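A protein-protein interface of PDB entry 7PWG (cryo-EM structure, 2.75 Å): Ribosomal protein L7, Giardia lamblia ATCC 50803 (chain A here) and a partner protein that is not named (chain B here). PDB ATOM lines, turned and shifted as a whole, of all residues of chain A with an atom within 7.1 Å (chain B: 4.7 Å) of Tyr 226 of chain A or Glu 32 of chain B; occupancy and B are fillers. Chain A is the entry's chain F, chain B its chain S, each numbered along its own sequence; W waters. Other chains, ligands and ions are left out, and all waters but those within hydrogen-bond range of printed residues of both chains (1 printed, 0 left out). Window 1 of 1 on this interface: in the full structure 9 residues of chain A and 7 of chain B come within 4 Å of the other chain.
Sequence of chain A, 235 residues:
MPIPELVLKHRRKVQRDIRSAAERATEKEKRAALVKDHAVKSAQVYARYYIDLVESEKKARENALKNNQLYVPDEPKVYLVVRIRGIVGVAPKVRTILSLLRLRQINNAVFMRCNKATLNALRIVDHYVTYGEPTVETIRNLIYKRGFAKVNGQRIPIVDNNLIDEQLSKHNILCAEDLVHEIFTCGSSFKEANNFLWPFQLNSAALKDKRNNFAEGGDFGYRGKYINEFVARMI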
ATOM      1  N   TYR A 131      26.074   7.433 -14.642  1.00  0.00           N
ATOM      2  CA  TYR A 131      27.410   7.904 -14.975  1.00  0.00           C
ATOM      3  C   TYR A 131      27.447   8.483 -16.380  1.00  0.00           C
ATOM      4  O   TYR A 131      26.568   8.230 -17.199  1.00  0.00           O
ATOM      5  CB  TYR A 131      28.446   6.784 -14.829  1.00  0.00           C
ATOM      6  CG  TYR A 131      28.120   5.538 -15.595  1.00  0.00           C
ATOM      7  CD1 TYR A 131      27.214   4.625 -15.103  1.00  0.00           C
ATOM      8  CD2 TYR A 131      28.711   5.275 -16.819  1.00  0.00           C
ATOM      9  CE1 TYR A 131      26.922   3.512 -15.783  1.00  0.00           C
ATOM     10  CE2 TYR A 131      28.427   4.149 -17.494  1.00  0.00           C
ATOM     11  CZ  TYR A 131      27.522   3.273 -16.974  1.00  0.00           C
ATOM     12  OH  TYR A 131      27.206   2.138 -17.655  1.00  0.00           O
ATOM     13  N   GLY A 132      28.498   9.244 -16.647  1.00  0.00           N
ATOM     14  CA  GLY A 132      28.675   9.851 -17.948  1.00  0.00           C
ATOM     15  C   GLY A 132      29.933  10.686 -17.985  1.00  0.00           C
ATOM     16  O   GLY A 132      30.837  10.495 -17.178  1.00  0.00           O
ATOM     17  N   GLU A 133      29.973  11.641 -18.911  1.00  0.00           N
ATOM     18  CA  GLU A 133      31.192  12.383 -19.215  1.00  0.00           C
ATOM     19  C   GLU A 133      31.119  13.822 -18.723  1.00  0.00           C
ATOM     20  O   GLU A 133      30.233  14.571 -19.151  1.00  0.00           O
ATOM     21  CB  GLU A 133      31.446  12.354 -20.720  1.00  0.00           C
ATOM     22  CG  GLU A 133      31.575  10.972 -21.281  1.00  0.00           C
ATOM     23  CD  GLU A 133      30.422  10.578 -22.188  1.00  0.00           C
ATOM     24  OE1 GLU A 133      29.899  11.446 -22.918  1.00  0.00           O
ATOM     25  OE2 GLU A 133      30.038   9.392 -22.171  1.00  0.00           O
ATOM     26  N   PHE A 214      18.280   4.366 -18.088  1.00  0.00           N
ATOM     27  CA  PHE A 214      18.077   5.688 -18.675  1.00  0.00           C
ATOM     28  C   PHE A 214      17.606   5.604 -20.113  1.00  0.00           C
ATOM     29  O   PHE A 214      16.952   6.526 -20.598  1.00  0.00           O
ATOM     30  CB  PHE A 214      19.369   6.509 -18.598  1.00  0.00           C
ATOM     31  CG  PHE A 214      19.234   7.928 -19.109  1.00  0.00           C
ATOM     32  CD1 PHE A 214      18.789   8.933 -18.283  1.00  0.00           C
ATOM     33  CD2 PHE A 214      19.577   8.254 -20.406  1.00  0.00           C
ATOM     34  CE1 PHE A 214      18.671  10.223 -18.737  1.00  0.00           C
ATOM     35  CE2 PHE A 214      19.460   9.542 -20.861  1.00  0.00           C
ATOM     36  CZ  PHE A 214      19.005  10.529 -20.023  1.00  0.00           C
ATOM     37  N   ARG A 223      24.295   7.759 -19.133  1.00  0.00           N
ATOM     38  CA  ARG A 223      23.504   8.874 -19.641  1.00  0.00           C
ATOM     39  C   ARG A 223      24.332   9.954 -20.321  1.00  0.00           C
ATOM     40  O   ARG A 223      23.796  11.018 -20.620  1.00  0.00           O
ATOM     41  CB  ARG A 223      22.649   9.498 -18.541  1.00  0.00           C
ATOM     42  CG  ARG A 223      23.364  10.387 -17.578  1.00  0.00           C
ATOM     43  CD  ARG A 223      22.353  11.142 -16.794  1.00  0.00           C
ATOM     44  NE  ARG A 223      21.599  10.266 -15.929  1.00  0.00           N
ATOM     45  CZ  ARG A 223      20.398  10.538 -15.446  1.00  0.00           C
ATOM     46  NH1 ARG A 223      19.789  11.657 -15.772  1.00  0.00           N
ATOM     47  NH2 ARG A 223      19.798   9.674 -14.661  1.00  0.00           N
ATOM     48  N   GLY A 224      25.603   9.699 -20.603  1.00  0.00           N
ATOM     49  CA  GLY A 224      26.346  10.560 -21.503  1.00  0.00           C
ATOM     50  C   GLY A 224      26.561  11.960 -20.972  1.00  0.00           C
ATOM     51  O   GLY A 224      26.861  12.174 -19.795  1.00  0.00           O
ATOM     52  N   LYS A 225      26.428  12.937 -21.861  1.00  0.00           N
ATOM     53  CA  LYS A 225      26.605  14.334 -21.486  1.00  0.00           C
ATOM     54  C   LYS A 225      25.492  14.854 -20.587  1.00  0.00           C
ATOM     55  O   LYS A 225      25.658  15.916 -19.988  1.00  0.00           O
ATOM     56  CB  LYS A 225      26.698  15.185 -22.742  1.00  0.00           C
ATOM     57  CG  LYS A 225      25.466  15.108 -23.588  1.00  0.00           C
ATOM     58  CD  LYS A 225      25.701  15.696 -24.936  1.00  0.00           C
ATOM     59  CE  LYS A 225      24.548  16.581 -25.346  1.00  0.00           C
ATOM     60  NZ  LYS A 225      24.303  17.634 -24.333  1.00  0.00           N
ATOM     61  N   TYR A 226      24.378  14.137 -20.472  1.00  0.00           N
ATOM     62  CA  TYR A 226      23.288  14.485 -19.575  1.00  0.00           C
ATOM     63  C   TYR A 226      23.636  14.278 -18.106  1.00  0.00           C
ATOM     64  O   TYR A 226      22.783  14.519 -17.253  1.00  0.00           O
ATOM     65  CB  TYR A 226      22.032  13.678 -19.935  1.00  0.00           C
ATOM     66  CG  TYR A 226      21.549  13.906 -21.357  1.00  0.00           C
ATOM     67  CD1 TYR A 226      21.204  15.171 -21.806  1.00  0.00           C
ATOM     68  CD2 TYR A 226      21.442  12.853 -22.242  1.00  0.00           C
ATOM     69  CE1 TYR A 226      20.784  15.373 -23.100  1.00  0.00           C
ATOM     70  CE2 TYR A 226      21.023  13.039 -23.526  1.00  0.00           C
ATOM     71  CZ  TYR A 226      20.690  14.298 -23.955  1.00  0.00           C
ATOM     72  OH  TYR A 226      20.273  14.468 -25.249  1.00  0.00           O
ATOM     73  N   ILE A 227      24.854  13.846 -17.785  1.00  0.00           N
ATOM     74  CA  ILE A 227      25.285  13.793 -16.397  1.00  0.00           C
ATOM     75  C   ILE A 227      25.529  15.190 -15.839  1.00  0.00           C
ATOM     76  O   ILE A 227      25.581  15.361 -14.621  1.00  0.00           O
ATOM     77  CB  ILE A 227      26.540  12.896 -16.268  1.00  0.00           C
ATOM     78  CG1 ILE A 227      26.710  12.373 -14.845  1.00  0.00           C
ATOM     79  CG2 ILE A 227      27.794  13.631 -16.680  1.00  0.00           C
ATOM     80  CD1 ILE A 227      25.536  11.581 -14.344  1.00  0.00           C
ATOM     81  N   ASN A 228      25.655  16.203 -16.697  1.00  0.00           N
ATOM     82  CA  ASN A 228      26.102  17.518 -16.248  1.00  0.00           C
ATOM     83  C   ASN A 228      24.979  18.342 -15.632  1.00  0.00           C
ATOM     84  O   ASN A 228      25.222  19.113 -14.700  1.00  0.00           O
ATOM     85  CB  ASN A 228      26.749  18.266 -17.407  1.00  0.00           C
ATOM     86  CG  ASN A 228      28.116  17.736 -17.732  1.00  0.00           C
ATOM     87  OD1 ASN A 228      28.937  17.565 -16.854  1.00  0.00           O
ATOM     88  ND2 ASN A 228      28.350  17.429 -18.989  1.00  0.00           N
ATOM     89  N   GLU A 229      23.759  18.210 -16.139  1.00  0.00           N
ATOM     90  CA  GLU A 229      22.607  18.844 -15.519  1.00  0.00           C
ATOM     91  C   GLU A 229      21.976  17.999 -14.424  1.00  0.00           C
ATOM     92  O   GLU A 229      21.215  18.534 -13.614  1.00  0.00           O
ATOM     93  CB  GLU A 229      21.565  19.174 -16.581  1.00  0.00           C
ATOM     94  CG  GLU A 229      21.331  18.045 -17.557  1.00  0.00           C
ATOM     95  CD  GLU A 229      20.655  18.501 -18.829  1.00  0.00           C
ATOM     96  OE1 GLU A 229      19.429  18.293 -18.962  1.00  0.00           O
ATOM     97  OE2 GLU A 229      21.347  19.074 -19.696  1.00  0.00           O
ATOM     98  N   PHE A 230      22.262  16.694 -14.392  1.00  0.00           N
ATOM     99  CA  PHE A 230      21.846  15.864 -13.271  1.00  0.00           C
ATOM    100  C   PHE A 230      22.542  16.301 -11.992  1.00  0.00           C
ATOM    101  O   PHE A 230      21.891  16.548 -10.973  1.00  0.00           O
ATOM    102  CB  PHE A 230      22.132  14.393 -13.581  1.00  0.00           C
ATOM    103  CG  PHE A 230      21.868  13.458 -12.437  1.00  0.00           C
ATOM    104  CD1 PHE A 230      20.589  13.217 -12.000  1.00  0.00           C
ATOM    105  CD2 PHE A 230      22.905  12.803 -11.817  1.00  0.00           C
ATOM    106  CE1 PHE A 230      20.361  12.362 -10.958  1.00  0.00           C
ATOM    107  CE2 PHE A 230      22.672  11.944 -10.784  1.00  0.00           C
ATOM    108  CZ  PHE A 230      21.409  11.724 -10.352  1.00  0.00           C
ATOM    109  N   VAL A 231      23.866  16.454 -12.033  1.00  0.00           N
ATOM    110  CA  VAL A 231      24.577  16.850 -10.823  1.00  0.00           C
ATOM    111  C   VAL A 231      24.589  18.348 -10.606  1.00  0.00           C
ATOM    112  O   VAL A 231      25.002  18.787  -9.535  1.00  0.00           O
ATOM    113  CB  VAL A 231      26.043  16.375 -10.779  1.00  0.00           C
ATOM    114  CG1 VAL A 231      26.106  14.864 -10.743  1.00  0.00           C
ATOM    115  CG2 VAL A 231      26.815  16.926 -11.936  1.00  0.00           C
ATOM    116  N   TYR B   5      17.183  12.101 -35.890  1.00  0.00           N
ATOM    117  CA  TYR B   5      18.617  11.852 -35.817  1.00  0.00           C
ATOM    118  C   TYR B   5      19.060  10.979 -36.984  1.00  0.00           C
ATOM    119  O   TYR B   5      18.329  10.094 -37.422  1.00  0.00           O
ATOM    120  CB  TYR B   5      19.027  11.153 -34.514  1.00  0.00           C
ATOM    121  CG  TYR B   5      18.839  11.939 -33.245  1.00  0.00           C
ATOM    122  CD1 TYR B   5      19.766  12.879 -32.848  1.00  0.00           C
ATOM    123  CD2 TYR B   5      17.742  11.718 -32.431  1.00  0.00           C
ATOM    124  CE1 TYR B   5      19.599  13.576 -31.694  1.00  0.00           C
ATOM    125  CE2 TYR B   5      17.571  12.417 -31.281  1.00  0.00           C
ATOM    126  CZ  TYR B   5      18.506  13.341 -30.908  1.00  0.00           C
ATOM    127  OH  TYR B   5      18.339  14.058 -29.748  1.00  0.00           O
ATOM    128  N   ASN B  31      16.080  11.703 -27.216  1.00  0.00           N
ATOM    129  CA  ASN B  31      17.403  12.303 -27.053  1.00  0.00           C
ATOM    130  C   ASN B  31      18.445  11.402 -27.701  1.00  0.00           C
ATOM    131  O   ASN B  31      18.123  10.362 -28.281  1.00  0.00           O
ATOM    132  CB  ASN B  31      17.745  12.572 -25.584  1.00  0.00           C
ATOM    133  CG  ASN B  31      17.572  11.362 -24.699  1.00  0.00           C
ATOM    134  OD1 ASN B  31      18.275  10.369 -24.834  1.00  0.00           O
ATOM    135  ND2 ASN B  31      16.647  11.455 -23.760  1.00  0.00           N
ATOM    136  N   GLU B  32      19.710  11.829 -27.590  1.00  0.00           N
ATOM    137  CA  GLU B  32      20.832  11.198 -28.279  1.00  0.00           C
ATOM    138  C   GLU B  32      21.195   9.846 -27.685  1.00  0.00           C
ATOM    139  O   GLU B  32      21.718   8.985 -28.393  1.00  0.00           O
ATOM    140  CB  GLU B  32      22.052  12.124 -28.233  1.00  0.00           C
ATOM    141  CG  GLU B  32      21.970  13.337 -29.175  1.00  0.00           C
ATOM    142  CD  GLU B  32      22.211  14.695 -28.501  1.00  0.00           C
ATOM    143  OE1 GLU B  32      22.739  14.731 -27.369  1.00  0.00           O
ATOM    144  OE2 GLU B  32      21.866  15.731 -29.118  1.00  0.00           O
ATOM    145  N   ILE B  33      20.953   9.642 -26.397  1.00  0.00           N
ATOM    146  CA  ILE B  33      21.298   8.370 -25.778  1.00  0.00           C
ATOM    147  C   ILE B  33      20.305   7.274 -26.172  1.00  0.00           C
ATOM    148  O   ILE B  33      20.692   6.130 -26.401  1.00  0.00           O
ATOM    149  CB  ILE B  33      21.418   8.563 -24.252  1.00  0.00           C
ATOM    150  CG1 ILE B  33      22.480   9.626 -23.942  1.00  0.00           C
ATOM    151  CG2 ILE B  33      21.760   7.283 -23.558  1.00  0.00           C
ATOM    152  CD1 ILE B  33      23.840   9.348 -24.499  1.00  0.00           C
ATOM    153  N   VAL B  34      19.019   7.595 -26.280  1.00  0.00           N
ATOM    154  CA  VAL B  34      18.050   6.607 -26.749  1.00  0.00           C
ATOM    155  C   VAL B  34      18.254   6.306 -28.229  1.00  0.00           C
ATOM    156  O   VAL B  34      18.082   5.170 -28.670  1.00  0.00           O
ATOM    157  CB  VAL B  34      16.613   7.075 -26.465  1.00  0.00           C
ATOM    158  CG1 VAL B  34      15.605   6.080 -27.023  1.00  0.00           C
ATOM    159  CG2 VAL B  34      16.409   7.254 -24.994  1.00  0.00           C
ATOM    160  N   ALA B  35      18.617   7.313 -29.019  1.00  0.00           N
ATOM    161  CA  ALA B  35      18.743   7.108 -30.456  1.00  0.00           C
ATOM    162  C   ALA B  35      19.883   6.156 -30.800  1.00  0.00           C
ATOM    163  O   ALA B  35      19.723   5.291 -31.665  1.00  0.00           O
ATOM    164  CB  ALA B  35      18.922   8.452 -31.155  1.00  0.00           C
ATOM    165  N   LYS B  36      21.041   6.291 -30.142  1.00  0.00           N
ATOM    166  CA  LYS B  36      22.165   5.404 -30.439  1.00  0.00           C
ATOM    167  C   LYS B  36      21.885   3.975 -30.015  1.00  0.00           C
ATOM    168  O   LYS B  36      22.373   3.039 -30.646  1.00  0.00           O
ATOM    169  CB  LYS B  36      23.449   5.891 -29.769  1.00  0.00           C
ATOM    170  CG  LYS B  36      24.137   7.008 -30.497  1.00  0.00           C
ATOM    171  CD  LYS B  36      25.443   7.428 -29.838  1.00  0.00           C
ATOM    172  CE  LYS B  36      25.310   7.614 -28.348  1.00  0.00           C
ATOM    173  NZ  LYS B  36      24.121   8.410 -27.961  1.00  0.00           N
ATOM    174  N   CYS B  59      26.120  11.029 -34.602  1.00  0.00           N
ATOM    175  CA  CYS B  59      24.713  11.159 -34.241  1.00  0.00           C
ATOM    176  C   CYS B  59      24.253  12.548 -34.674  1.00  0.00           C
ATOM    177  O   CYS B  59      24.139  13.464 -33.866  1.00  0.00           O
ATOM    178  CB  CYS B  59      24.539  10.951 -32.790  1.00  0.00           C
ATOM    179  SG  CYS B  59      22.888  10.470 -32.281  1.00  0.00           S
HETATM  180  O   HOH W   1      16.185   8.877 -21.524  1.00  0.00           O
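OE1 of Glu 32 of chain B sits at hydrogen-bond distance from OH of Tyr 226 of chain A (3.3 Å).
The backbone NH of Glu 32 of chain B sits at hydrogen-bond distance from the side-chain hydroxyl of Tyr 5 of chain B, 3.4 Å away.
The backbone NH of Ile 33 of chain B lies within hydrogen-bond range of the side-chain amide oxygen of Asn 31 of chain B (3.2 Å).
OD1 of Asn 31 of chain B is in hydrogen-bond range of N of Val 34 of chain B (3.2 Å).
The backbone carbonyl oxygen (O) of Glu 32 of chain B lies within hydrogen-bond range of the side-chain amino group (NZ) of Lys 36 of chain B, at 2.5 Å.
O of Tyr 131 of chain A sits at hydrogen-bond distance from N of Arg 223 of chain A (3.0 Å).
The side-chain amide nitrogen of Asn 228 of chain A is in hydrogen-bond range of the backbone carbonyl oxygen of Lys 225 of chain A (3.2 Å).
Of the printed residues of chain A, Glu 32 of chain B touches Lys 225 (3.3 Å) and Tyr 226 (3.3 Å).
Printed residues of chain B within 4 Å of Arg 223 of chain A: Ile 33.
Of the printed residues of chain B, Lys 225 of chain A touches Glu 32 (3.3 Å).
Printed residues of chain A within 4 Å of Asn 31 of chain B: Tyr 226 (3.2 Å).
Printed residues of chain B within 4 Å of Phe 214 of chain A: Ile 33 (3.96 Å).
Of the printed residues of chain A, Ile 33 of chain B touches Phe 214, Arg 223 and Tyr 226.
Phe 230 of chain A touches none of the printed residues of chain B.
The nearest printed residue of chain B that does not touch Tyr 226 of chain A is Tyr 5 of chain B (4.9 Å).
The nearest residue of chain A that does not touch Glu 32 of chain B is Phe 214 of chain A (7.0 Å).
The nearest printed residue of chain B that does not touch Phe 214 of chain A is Asn 31 of chain B (4.2 Å).
Of the 13 printed residues of chain A, 4 touch a printed residue of chain B.
Of the 8 printed residues of chain B, 3 touch a printed residue of chain A.
Printed residues of chain B that touch a printed residue of chain A: Asn 31, Glu 32 and Ile 33.
Hydrophobic or aromatic side chains of chain B within 4 Å of the printed part of chain A: Ile 33.
Among the printed residues, 6 pairs touch across the chains.
Among the printed residues, no Asp or Glu carboxylate lies within 4 Å of a Lys or Arg side-chain nitrogen of the other chain.
Water W1 bridges O of Phe 214 of chain A and ND2 of Asn 31 of chain B.
Ile 33 of chain B touches Phe 214 of chain A (CG2 to CD2, 3.96 Å).
Arg 223 of chain A touches Ile 33 of chain B (O to CG1, 3.8 Å).
Glu 32 of chain B touches Lys 225 of chain A (OE1 to CE, 3.3 Å).
Tyr 226 of chain A touches Asn 31 of chain B.
CG1 of Ile 33 of chain B touches CE2 of Tyr 226 of chain A (3.7 Å).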
